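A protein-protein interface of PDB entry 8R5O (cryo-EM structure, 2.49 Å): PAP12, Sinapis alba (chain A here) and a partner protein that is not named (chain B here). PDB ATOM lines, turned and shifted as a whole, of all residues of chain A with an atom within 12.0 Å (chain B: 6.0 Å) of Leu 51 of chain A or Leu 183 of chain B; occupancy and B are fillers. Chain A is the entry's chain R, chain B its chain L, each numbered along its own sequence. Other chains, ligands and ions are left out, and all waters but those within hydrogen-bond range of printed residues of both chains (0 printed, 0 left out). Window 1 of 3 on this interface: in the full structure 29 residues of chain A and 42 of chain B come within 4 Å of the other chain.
N of Leu 51 of chain A is in hydrogen-bond range of OD2 of Asp 76 of chain B, 3.3 Å away. The guanidinium group (NH2) of Arg 86 of chain B is in salt-bridge range of the side-chain carboxylate (OD1) of Asp 55 of chain A. The side-chain sulfur of Met 57 of chain A lies within hydrogen-bond range of the guanidinium group of Arg 86 of chain B, at 3.2 Å. O of Lys 54 of chain A is in hydrogen-bond range of NH2 of Arg 182 of chain B, 3.3 Å away. O of Leu 51 of chain A lies close to OD2 of Asp 186 of chain B (2.7 Å). O of Phe 187 of chain B is in hydrogen-bond range of NH1 of Arg 49 of chain A (2.9 Å).
The backbone carbonyl oxygen (O) of Ile 82 of chain B sits at hydrogen-bond distance from the guanidinium group (NH1) of Arg 86 of chain B, 2.9 Å away. The backbone NH (N) of Met 57 of chain A sits close to the side-chain carboxylate (OD1) of Asp 55 of chain A, 3.2 Å away.
Asp 76 of chain B touches Arg 49 of chain A. Asp 186 of chain B touches Arg 49 of chain A. Asp 186 of chain B touches Thr 50 of chain A (CB to O, 3.5 Å). Leu 51 of chain A touches Asp 78 of chain B. O of Leu 183 of chain B touches CD1 of Leu 51 of chain A, 3.8 Å away. Leu 51 of chain A touches Phe 187 of chain B (N to CZ, 3.6 Å). CG of Asp 186 of chain B touches CG2 of Thr 52 of chain A, 3.6 Å away. Asp 186 of chain B touches Lys 53 of chain A (OD2 to CE, 3.2 Å). Asp 55 of chain A touches Ile 82 of chain B (OD2 to CG2, 3.4 Å). Leu 58 of chain A touches Ile 82 of chain B.
Leu 51 of chain A touches just these residues of chain B: Asp 76 (3.3 Å), Asp 78 (3.8 Å), Ile 82 (3.8 Å), Leu 183 (3.8 Å), Asp 186 (2.7 Å) and Phe 187 (3.6 Å). Leu 183 of chain B touches three residues of chain A. Asp 76 of chain B touches three residues of chain A. Ile 82 of chain B touches just these residues of chain A: Leu 51, Asp 55 and Leu 58. No residue of chain A comes within 4 Å of Phe 180 of chain B. No residue of chain A comes within 4 Å of Gly 185 of chain B. Printed residues of chain B within 4 Å of Lys 54 of chain A: Arg 182 and Leu 183. Of the printed residues of chain B, Arg 49 of chain A touches Asp 76 (3.7 Å), Asp 186 (3.99 Å) and Phe 187 (2.9 Å). Arg 47 of chain A touches none of the printed residues of chain B. Tyr 184 of chain B touches none of the printed residues of chain A.
Of the 13 printed residues of chain B, 8 touch a printed residue of chain A. Hydrophobic or aromatic side chains of chain B that line the printed part of chain A: Ile 82, Leu 183 and Phe 187. Of the 12 printed residues of chain A, 9 touch a printed residue of chain B. Printed residues of chain A that touch a printed residue of chain B: Arg 49, Thr 50, Leu 51, Thr 52, Lys 53, Lys 54, Asp 55, Met 57 and Leu 58. Hydrophobic or aromatic side chains of chain A within 4 Å of the printed part of chain B: Leu 51, Met 57 and Leu 58.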
ATOM      1  N   ARG A  47      10.628  16.173   3.973  1.00  0.00           N
ATOM      2  CA  ARG A  47       9.646  16.143   5.048  1.00  0.00           C
ATOM      3  C   ARG A  47       8.486  15.243   4.643  1.00  0.00           C
ATOM      4  O   ARG A  47       7.766  15.542   3.685  1.00  0.00           O
ATOM      5  CB  ARG A  47       9.162  17.560   5.356  1.00  0.00           C
ATOM      6  CG  ARG A  47       8.410  17.707   6.666  1.00  0.00           C
ATOM      7  CD  ARG A  47       6.915  17.606   6.464  1.00  0.00           C
ATOM      8  NE  ARG A  47       6.432  18.569   5.481  1.00  0.00           N
ATOM      9  CZ  ARG A  47       5.154  18.746   5.178  1.00  0.00           C
ATOM     10  NH1 ARG A  47       4.201  18.047   5.770  1.00  0.00           N
ATOM     11  NH2 ARG A  47       4.825  19.648   4.257  1.00  0.00           N
ATOM     12  N   ARG A  48       8.308  14.143   5.369  1.00  0.00           N
ATOM     13  CA  ARG A  48       7.184  13.255   5.111  1.00  0.00           C
ATOM     14  C   ARG A  48       5.896  13.893   5.608  1.00  0.00           C
ATOM     15  O   ARG A  48       5.834  14.402   6.730  1.00  0.00           O
ATOM     16  CB  ARG A  48       7.396  11.901   5.789  1.00  0.00           C
ATOM     17  CG  ARG A  48       8.269  10.925   5.016  1.00  0.00           C
ATOM     18  CD  ARG A  48       9.729  11.335   5.037  1.00  0.00           C
ATOM     19  NE  ARG A  48      10.605  10.264   4.580  1.00  0.00           N
ATOM     20  CZ  ARG A  48      11.916  10.388   4.419  1.00  0.00           C
ATOM     21  NH1 ARG A  48      12.534  11.534   4.648  1.00  0.00           N
ATOM     22  NH2 ARG A  48      12.622   9.336   4.017  1.00  0.00           N
ATOM     23  N   ARG A  49       4.865  13.866   4.770  1.00  0.00           N
ATOM     24  CA  ARG A  49       3.588  14.462   5.131  1.00  0.00           C
ATOM     25  C   ARG A  49       2.773  13.476   5.958  1.00  0.00           C
ATOM     26  O   ARG A  49       2.662  12.298   5.606  1.00  0.00           O
ATOM     27  CB  ARG A  49       2.826  14.874   3.875  1.00  0.00           C
ATOM     28  CG  ARG A  49       3.630  15.764   2.945  1.00  0.00           C
ATOM     29  CD  ARG A  49       2.871  16.027   1.664  1.00  0.00           C
ATOM     30  NE  ARG A  49       3.706  16.631   0.635  1.00  0.00           N
ATOM     31  CZ  ARG A  49       3.346  16.755  -0.635  1.00  0.00           C
ATOM     32  NH1 ARG A  49       2.172  16.326  -1.065  1.00  0.00           N
ATOM     33  NH2 ARG A  49       4.188  17.319  -1.495  1.00  0.00           N
ATOM     34  N   THR A  50       2.209  13.961   7.058  1.00  0.00           N
ATOM     35  CA  THR A  50       1.451  13.123   7.973  1.00  0.00           C
ATOM     36  C   THR A  50       0.158  13.832   8.342  1.00  0.00           C
ATOM     37  O   THR A  50      -0.037  15.013   8.046  1.00  0.00           O
ATOM     38  CB  THR A  50       2.257  12.782   9.234  1.00  0.00           C
ATOM     39  OG1 THR A  50       3.251  13.790   9.458  1.00  0.00           O
ATOM     40  CG2 THR A  50       2.931  11.429   9.085  1.00  0.00           C
ATOM     41  N   LEU A  51      -0.733  13.088   8.997  1.00  0.00           N
ATOM     42  CA  LEU A  51      -2.052  13.622   9.310  1.00  0.00           C
ATOM     43  C   LEU A  51      -1.964  14.806  10.267  1.00  0.00           C
ATOM     44  O   LEU A  51      -2.728  15.766  10.130  1.00  0.00           O
ATOM     45  CB  LEU A  51      -2.941  12.522   9.888  1.00  0.00           C
ATOM     46  CG  LEU A  51      -4.424  12.861  10.010  1.00  0.00           C
ATOM     47  CD1 LEU A  51      -4.910  13.613   8.781  1.00  0.00           C
ATOM     48  CD2 LEU A  51      -5.231  11.594  10.209  1.00  0.00           C
ATOM     49  N   THR A  52      -1.047  14.745  11.241  1.00  0.00           N
ATOM     50  CA  THR A  52      -0.774  15.799  12.223  1.00  0.00           C
ATOM     51  C   THR A  52      -2.051  16.494  12.687  1.00  0.00           C
ATOM     52  O   THR A  52      -2.080  17.715  12.873  1.00  0.00           O
ATOM     53  CB  THR A  52       0.246  16.821  11.679  1.00  0.00           C
ATOM     54  OG1 THR A  52       0.527  17.801  12.687  1.00  0.00           O
ATOM     55  CG2 THR A  52      -0.236  17.534  10.411  1.00  0.00           C
ATOM     56  N   LYS A  53      -3.101  15.707  12.899  1.00  0.00           N
ATOM     57  CA  LYS A  53      -4.441  16.185  13.203  1.00  0.00           C
ATOM     58  C   LYS A  53      -5.287  14.961  13.514  1.00  0.00           C
ATOM     59  O   LYS A  53      -4.974  13.848  13.078  1.00  0.00           O
ATOM     60  CB  LYS A  53      -5.039  16.984  12.039  1.00  0.00           C
ATOM     61  CG  LYS A  53      -6.221  17.855  12.411  1.00  0.00           C
ATOM     62  CD  LYS A  53      -6.650  18.715  11.236  1.00  0.00           C
ATOM     63  CE  LYS A  53      -5.589  19.740  10.885  1.00  0.00           C
ATOM     64  NZ  LYS A  53      -5.324  20.661  12.020  1.00  0.00           N
ATOM     65  N   LYS A  54      -6.357  15.169  14.271  1.00  0.00           N
ATOM     66  CA  LYS A  54      -7.144  14.071  14.813  1.00  0.00           C
ATOM     67  C   LYS A  54      -8.395  13.861  13.968  1.00  0.00           C
ATOM     68  O   LYS A  54      -9.183  14.791  13.771  1.00  0.00           O
ATOM     69  CB  LYS A  54      -7.512  14.345  16.271  1.00  0.00           C
ATOM     70  CG  LYS A  54      -7.494  13.108  17.161  1.00  0.00           C
ATOM     71  CD  LYS A  54      -6.165  12.363  17.060  1.00  0.00           C
ATOM     72  CE  LYS A  54      -4.985  13.236  17.474  1.00  0.00           C
ATOM     73  NZ  LYS A  54      -5.036  13.627  18.910  1.00  0.00           N
ATOM     74  N   ASP A  55      -8.567  12.639  13.469  1.00  0.00           N
ATOM     75  CA  ASP A  55      -9.767  12.228  12.751  1.00  0.00           C
ATOM     76  C   ASP A  55     -10.462  11.160  13.587  1.00  0.00           C
ATOM     77  O   ASP A  55      -9.965  10.035  13.702  1.00  0.00           O
ATOM     78  CB  ASP A  55      -9.427  11.702  11.358  1.00  0.00           C
ATOM     79  CG  ASP A  55     -10.658  11.273  10.576  1.00  0.00           C
ATOM     80  OD1 ASP A  55     -11.770  11.740  10.902  1.00  0.00           O
ATOM     81  OD2 ASP A  55     -10.515  10.464   9.637  1.00  0.00           O
ATOM     82  N   ASP A  56     -11.605  11.514  14.173  1.00  0.00           N
ATOM     83  CA  ASP A  56     -12.339  10.565  15.000  1.00  0.00           C
ATOM     84  C   ASP A  56     -13.025   9.480  14.184  1.00  0.00           C
ATOM     85  O   ASP A  56     -13.447   8.472  14.762  1.00  0.00           O
ATOM     86  CB  ASP A  56     -13.366  11.305  15.857  1.00  0.00           C
ATOM     87  CG  ASP A  56     -12.719  12.249  16.853  1.00  0.00           C
ATOM     88  OD1 ASP A  56     -11.607  11.939  17.332  1.00  0.00           O
ATOM     89  OD2 ASP A  56     -13.320  13.301  17.157  1.00  0.00           O
ATOM     90  N   MET A  57     -13.148   9.655  12.868  1.00  0.00           N
ATOM     91  CA  MET A  57     -13.744   8.628  12.024  1.00  0.00           C
ATOM     92  C   MET A  57     -12.827   7.432  11.805  1.00  0.00           C
ATOM     93  O   MET A  57     -13.304   6.388  11.348  1.00  0.00           O
ATOM     94  CB  MET A  57     -14.143   9.219  10.670  1.00  0.00           C
ATOM     95  CG  MET A  57     -15.301  10.199  10.733  1.00  0.00           C
ATOM     96  SD  MET A  57     -15.946  10.606   9.100  1.00  0.00           S
ATOM     97  CE  MET A  57     -16.368   8.978   8.488  1.00  0.00           C
ATOM     98  N   LEU A  58     -11.540   7.553  12.111  1.00  0.00           N
ATOM     99  CA  LEU A  58     -10.605   6.451  11.912  1.00  0.00           C
ATOM    100  C   LEU A  58     -10.786   5.372  12.975  1.00  0.00           C
ATOM    101  O   LEU A  58     -10.211   5.450  14.061  1.00  0.00           O
ATOM    102  CB  LEU A  58      -9.161   6.958  11.919  1.00  0.00           C
ATOM    103  CG  LEU A  58      -8.748   7.867  10.761  1.00  0.00           C
ATOM    104  CD1 LEU A  58      -7.243   8.054  10.744  1.00  0.00           C
ATOM    105  CD2 LEU A  58      -9.239   7.311   9.435  1.00  0.00           C
ATOM    106  N   ASP B  76       1.849   7.989   4.329  1.00  0.00           N
ATOM    107  CA  ASP B  76       1.284   7.774   5.650  1.00  0.00           C
ATOM    108  C   ASP B  76       0.044   6.890   5.531  1.00  0.00           C
ATOM    109  O   ASP B  76      -0.824   7.162   4.692  1.00  0.00           O
ATOM    110  CB  ASP B  76       0.922   9.122   6.280  1.00  0.00           C
ATOM    111  CG  ASP B  76       0.474   9.001   7.723  1.00  0.00           C
ATOM    112  OD1 ASP B  76       0.830   8.008   8.387  1.00  0.00           O
ATOM    113  OD2 ASP B  76      -0.241   9.908   8.197  1.00  0.00           O
ATOM    114  N   ASP B  78      -2.541   6.753   7.246  1.00  0.00           N
ATOM    115  CA  ASP B  78      -3.736   7.555   7.467  1.00  0.00           C
ATOM    116  C   ASP B  78      -4.125   8.395   6.258  1.00  0.00           C
ATOM    117  O   ASP B  78      -5.242   8.922   6.233  1.00  0.00           O
ATOM    118  CB  ASP B  78      -3.540   8.466   8.679  1.00  0.00           C
ATOM    119  CG  ASP B  78      -3.620   7.715   9.992  1.00  0.00           C
ATOM    120  OD1 ASP B  78      -3.934   6.506   9.969  1.00  0.00           O
ATOM    121  OD2 ASP B  78      -3.371   8.333  11.048  1.00  0.00           O
ATOM    122  N   ILE B  82      -8.284   8.175   5.772  1.00  0.00           N
ATOM    123  CA  ILE B  82      -9.250   9.248   5.994  1.00  0.00           C
ATOM    124  C   ILE B  82     -10.206   9.354   4.814  1.00  0.00           C
ATOM    125  O   ILE B  82     -11.391   9.661   4.986  1.00  0.00           O
ATOM    126  CB  ILE B  82      -8.537  10.583   6.280  1.00  0.00           C
ATOM    127  CG1 ILE B  82      -7.613  10.974   5.126  1.00  0.00           C
ATOM    128  CG2 ILE B  82      -7.769  10.502   7.590  1.00  0.00           C
ATOM    129  CD1 ILE B  82      -7.019  12.353   5.257  1.00  0.00           C
ATOM    130  N   ARG B  86     -14.501   7.499   4.215  1.00  0.00           N
ATOM    131  CA  ARG B  86     -15.470   8.388   3.589  1.00  0.00           C
ATOM    132  C   ARG B  86     -15.748   7.980   2.145  1.00  0.00           C
ATOM    133  O   ARG B  86     -16.037   8.830   1.302  1.00  0.00           O
ATOM    134  CB  ARG B  86     -14.992   9.835   3.664  1.00  0.00           C
ATOM    135  CG  ARG B  86     -14.881  10.366   5.079  1.00  0.00           C
ATOM    136  CD  ARG B  86     -14.099  11.663   5.125  1.00  0.00           C
ATOM    137  NE  ARG B  86     -14.136  12.275   6.447  1.00  0.00           N
ATOM    138  CZ  ARG B  86     -13.310  11.974   7.440  1.00  0.00           C
ATOM    139  NH1 ARG B  86     -12.361  11.065   7.297  1.00  0.00           N
ATOM    140  NH2 ARG B  86     -13.444  12.598   8.607  1.00  0.00           N
ATOM    141  N   HIS B 179     -15.095  19.879   7.629  1.00  0.00           N
ATOM    142  CA  HIS B 179     -14.702  19.718   6.236  1.00  0.00           C
ATOM    143  C   HIS B 179     -13.568  18.707   6.106  1.00  0.00           C
ATOM    144  O   HIS B 179     -12.676  18.635   6.955  1.00  0.00           O
ATOM    145  CB  HIS B 179     -14.285  21.059   5.639  1.00  0.00           C
ATOM    146  CG  HIS B 179     -14.420  21.120   4.150  1.00  0.00           C
ATOM    147  ND1 HIS B 179     -13.447  20.654   3.294  1.00  0.00           N
ATOM    148  CD2 HIS B 179     -15.420  21.585   3.365  1.00  0.00           C
ATOM    149  CE1 HIS B 179     -13.839  20.832   2.047  1.00  0.00           C
ATOM    150  NE2 HIS B 179     -15.033  21.396   2.061  1.00  0.00           N
ATOM    151  N   PHE B 180     -13.613  17.920   5.028  1.00  0.00           N
ATOM    152  CA  PHE B 180     -12.599  16.896   4.805  1.00  0.00           C
ATOM    153  C   PHE B 180     -11.223  17.499   4.563  1.00  0.00           C
ATOM    154  O   PHE B 180     -10.213  16.929   4.987  1.00  0.00           O
ATOM    155  CB  PHE B 180     -13.004  16.008   3.628  1.00  0.00           C
ATOM    156  CG  PHE B 180     -11.947  15.026   3.212  1.00  0.00           C
ATOM    157  CD1 PHE B 180     -11.652  13.930   4.003  1.00  0.00           C
ATOM    158  CD2 PHE B 180     -11.260  15.191   2.022  1.00  0.00           C
ATOM    159  CE1 PHE B 180     -10.686  13.024   3.622  1.00  0.00           C
ATOM    160  CE2 PHE B 180     -10.291  14.285   1.636  1.00  0.00           C
ATOM    161  CZ  PHE B 180     -10.004  13.201   2.438  1.00  0.00           C
ATOM    162  N   TRP B 181     -11.158  18.647   3.888  1.00  0.00           N
ATOM    163  CA  TRP B 181      -9.873  19.259   3.573  1.00  0.00           C
ATOM    164  C   TRP B 181      -9.175  19.835   4.797  1.00  0.00           C
ATOM    165  O   TRP B 181      -8.002  20.209   4.697  1.00  0.00           O
ATOM    166  CB  TRP B 181     -10.054  20.330   2.498  1.00  0.00           C
ATOM    167  CG  TRP B 181     -10.212  19.729   1.140  1.00  0.00           C
ATOM    168  CD1 TRP B 181     -11.293  19.045   0.672  1.00  0.00           C
ATOM    169  CD2 TRP B 181      -9.250  19.732   0.082  1.00  0.00           C
ATOM    170  NE1 TRP B 181     -11.069  18.628  -0.615  1.00  0.00           N
ATOM    171  CE2 TRP B 181      -9.821  19.037  -1.001  1.00  0.00           C
ATOM    172  CE3 TRP B 181      -7.962  20.259  -0.058  1.00  0.00           C
ATOM    173  CZ2 TRP B 181      -9.150  18.856  -2.207  1.00  0.00           C
ATOM    174  CZ3 TRP B 181      -7.300  20.077  -1.255  1.00  0.00           C
ATOM    175  CH2 TRP B 181      -7.894  19.382  -2.314  1.00  0.00           C
ATOM    176  N   ARG B 182      -9.855  19.917   5.941  1.00  0.00           N
ATOM    177  CA  ARG B 182      -9.147  20.161   7.192  1.00  0.00           C
ATOM    178  C   ARG B 182      -8.155  19.039   7.472  1.00  0.00           C
ATOM    179  O   ARG B 182      -7.034  19.288   7.929  1.00  0.00           O
ATOM    180  CB  ARG B 182     -10.145  20.302   8.342  1.00  0.00           C
ATOM    181  CG  ARG B 182      -9.522  20.735   9.657  1.00  0.00           C
ATOM    182  CD  ARG B 182     -10.520  20.656  10.803  1.00  0.00           C
ATOM    183  NE  ARG B 182     -10.842  19.277  11.155  1.00  0.00           N
ATOM    184  CZ  ARG B 182     -10.283  18.608  12.154  1.00  0.00           C
ATOM    185  NH1 ARG B 182      -9.379  19.167  12.942  1.00  0.00           N
ATOM    186  NH2 ARG B 182     -10.644  17.347  12.372  1.00  0.00           N
ATOM    187  N   LEU B 183      -8.553  17.796   7.198  1.00  0.00           N
ATOM    188  CA  LEU B 183      -7.649  16.659   7.323  1.00  0.00           C
ATOM    189  C   LEU B 183      -6.752  16.524   6.098  1.00  0.00           C
ATOM    190  O   LEU B 183      -5.543  16.309   6.224  1.00  0.00           O
ATOM    191  CB  LEU B 183      -8.453  15.375   7.526  1.00  0.00           C
ATOM    192  CG  LEU B 183      -9.420  15.354   8.705  1.00  0.00           C
ATOM    193  CD1 LEU B 183     -10.289  14.114   8.646  1.00  0.00           C
ATOM    194  CD2 LEU B 183      -8.652  15.413  10.010  1.00  0.00           C
ATOM    195  N   TYR B 184      -7.334  16.641   4.904  1.00  0.00           N
ATOM    196  CA  TYR B 184      -6.569  16.428   3.681  1.00  0.00           C
ATOM    197  C   TYR B 184      -5.550  17.535   3.448  1.00  0.00           C
ATOM    198  O   TYR B 184      -4.552  17.318   2.755  1.00  0.00           O
ATOM    199  CB  TYR B 184      -7.516  16.314   2.488  1.00  0.00           C
ATOM    200  CG  TYR B 184      -6.845  15.848   1.218  1.00  0.00           C
ATOM    201  CD1 TYR B 184      -6.584  14.504   1.004  1.00  0.00           C
ATOM    202  CD2 TYR B 184      -6.473  16.751   0.235  1.00  0.00           C
ATOM    203  CE1 TYR B 184      -5.972  14.072  -0.150  1.00  0.00           C
ATOM    204  CE2 TYR B 184      -5.857  16.327  -0.925  1.00  0.00           C
ATOM    205  CZ  TYR B 184      -5.610  14.985  -1.111  1.00  0.00           C
ATOM    206  OH  TYR B 184      -5.000  14.551  -2.261  1.00  0.00           O
ATOM    207  N   GLY B 185      -5.776  18.720   4.018  1.00  0.00           N
ATOM    208  CA  GLY B 185      -4.850  19.824   3.841  1.00  0.00           C
ATOM    209  C   GLY B 185      -3.468  19.568   4.403  1.00  0.00           C
ATOM    210  O   GLY B 185      -2.505  20.212   3.974  1.00  0.00           O
ATOM    211  N   ASP B 186      -3.344  18.637   5.351  1.00  0.00           N
ATOM    212  CA  ASP B 186      -2.048  18.311   5.931  1.00  0.00           C
ATOM    213  C   ASP B 186      -1.167  17.502   4.990  1.00  0.00           C
ATOM    214  O   ASP B 186       0.032  17.372   5.253  1.00  0.00           O
ATOM    215  CB  ASP B 186      -2.240  17.550   7.241  1.00  0.00           C
ATOM    216  CG  ASP B 186      -2.957  18.374   8.287  1.00  0.00           C
ATOM    217  OD1 ASP B 186      -2.596  19.556   8.465  1.00  0.00           O
ATOM    218  OD2 ASP B 186      -3.892  17.845   8.921  1.00  0.00           O
ATOM    219  N   PHE B 187      -1.725  16.958   3.913  1.00  0.00           N
ATOM    220  CA  PHE B 187      -0.950  16.253   2.906  1.00  0.00           C
ATOM    221  C   PHE B 187      -0.688  17.103   1.672  1.00  0.00           C
ATOM    222  O   PHE B 187      -0.120  16.602   0.701  1.00  0.00           O
ATOM    223  CB  PHE B 187      -1.660  14.956   2.512  1.00  0.00           C
ATOM    224  CG  PHE B 187      -1.889  14.024   3.664  1.00  0.00           C
ATOM    225  CD1 PHE B 187      -0.903  13.133   4.059  1.00  0.00           C
ATOM    226  CD2 PHE B 187      -3.085  14.044   4.362  1.00  0.00           C
ATOM    227  CE1 PHE B 187      -1.111  12.276   5.124  1.00  0.00           C
ATOM    228  CE2 PHE B 187      -3.297  13.191   5.426  1.00  0.00           C
ATOM    229  CZ  PHE B 187      -2.310  12.305   5.807  1.00  0.00           C
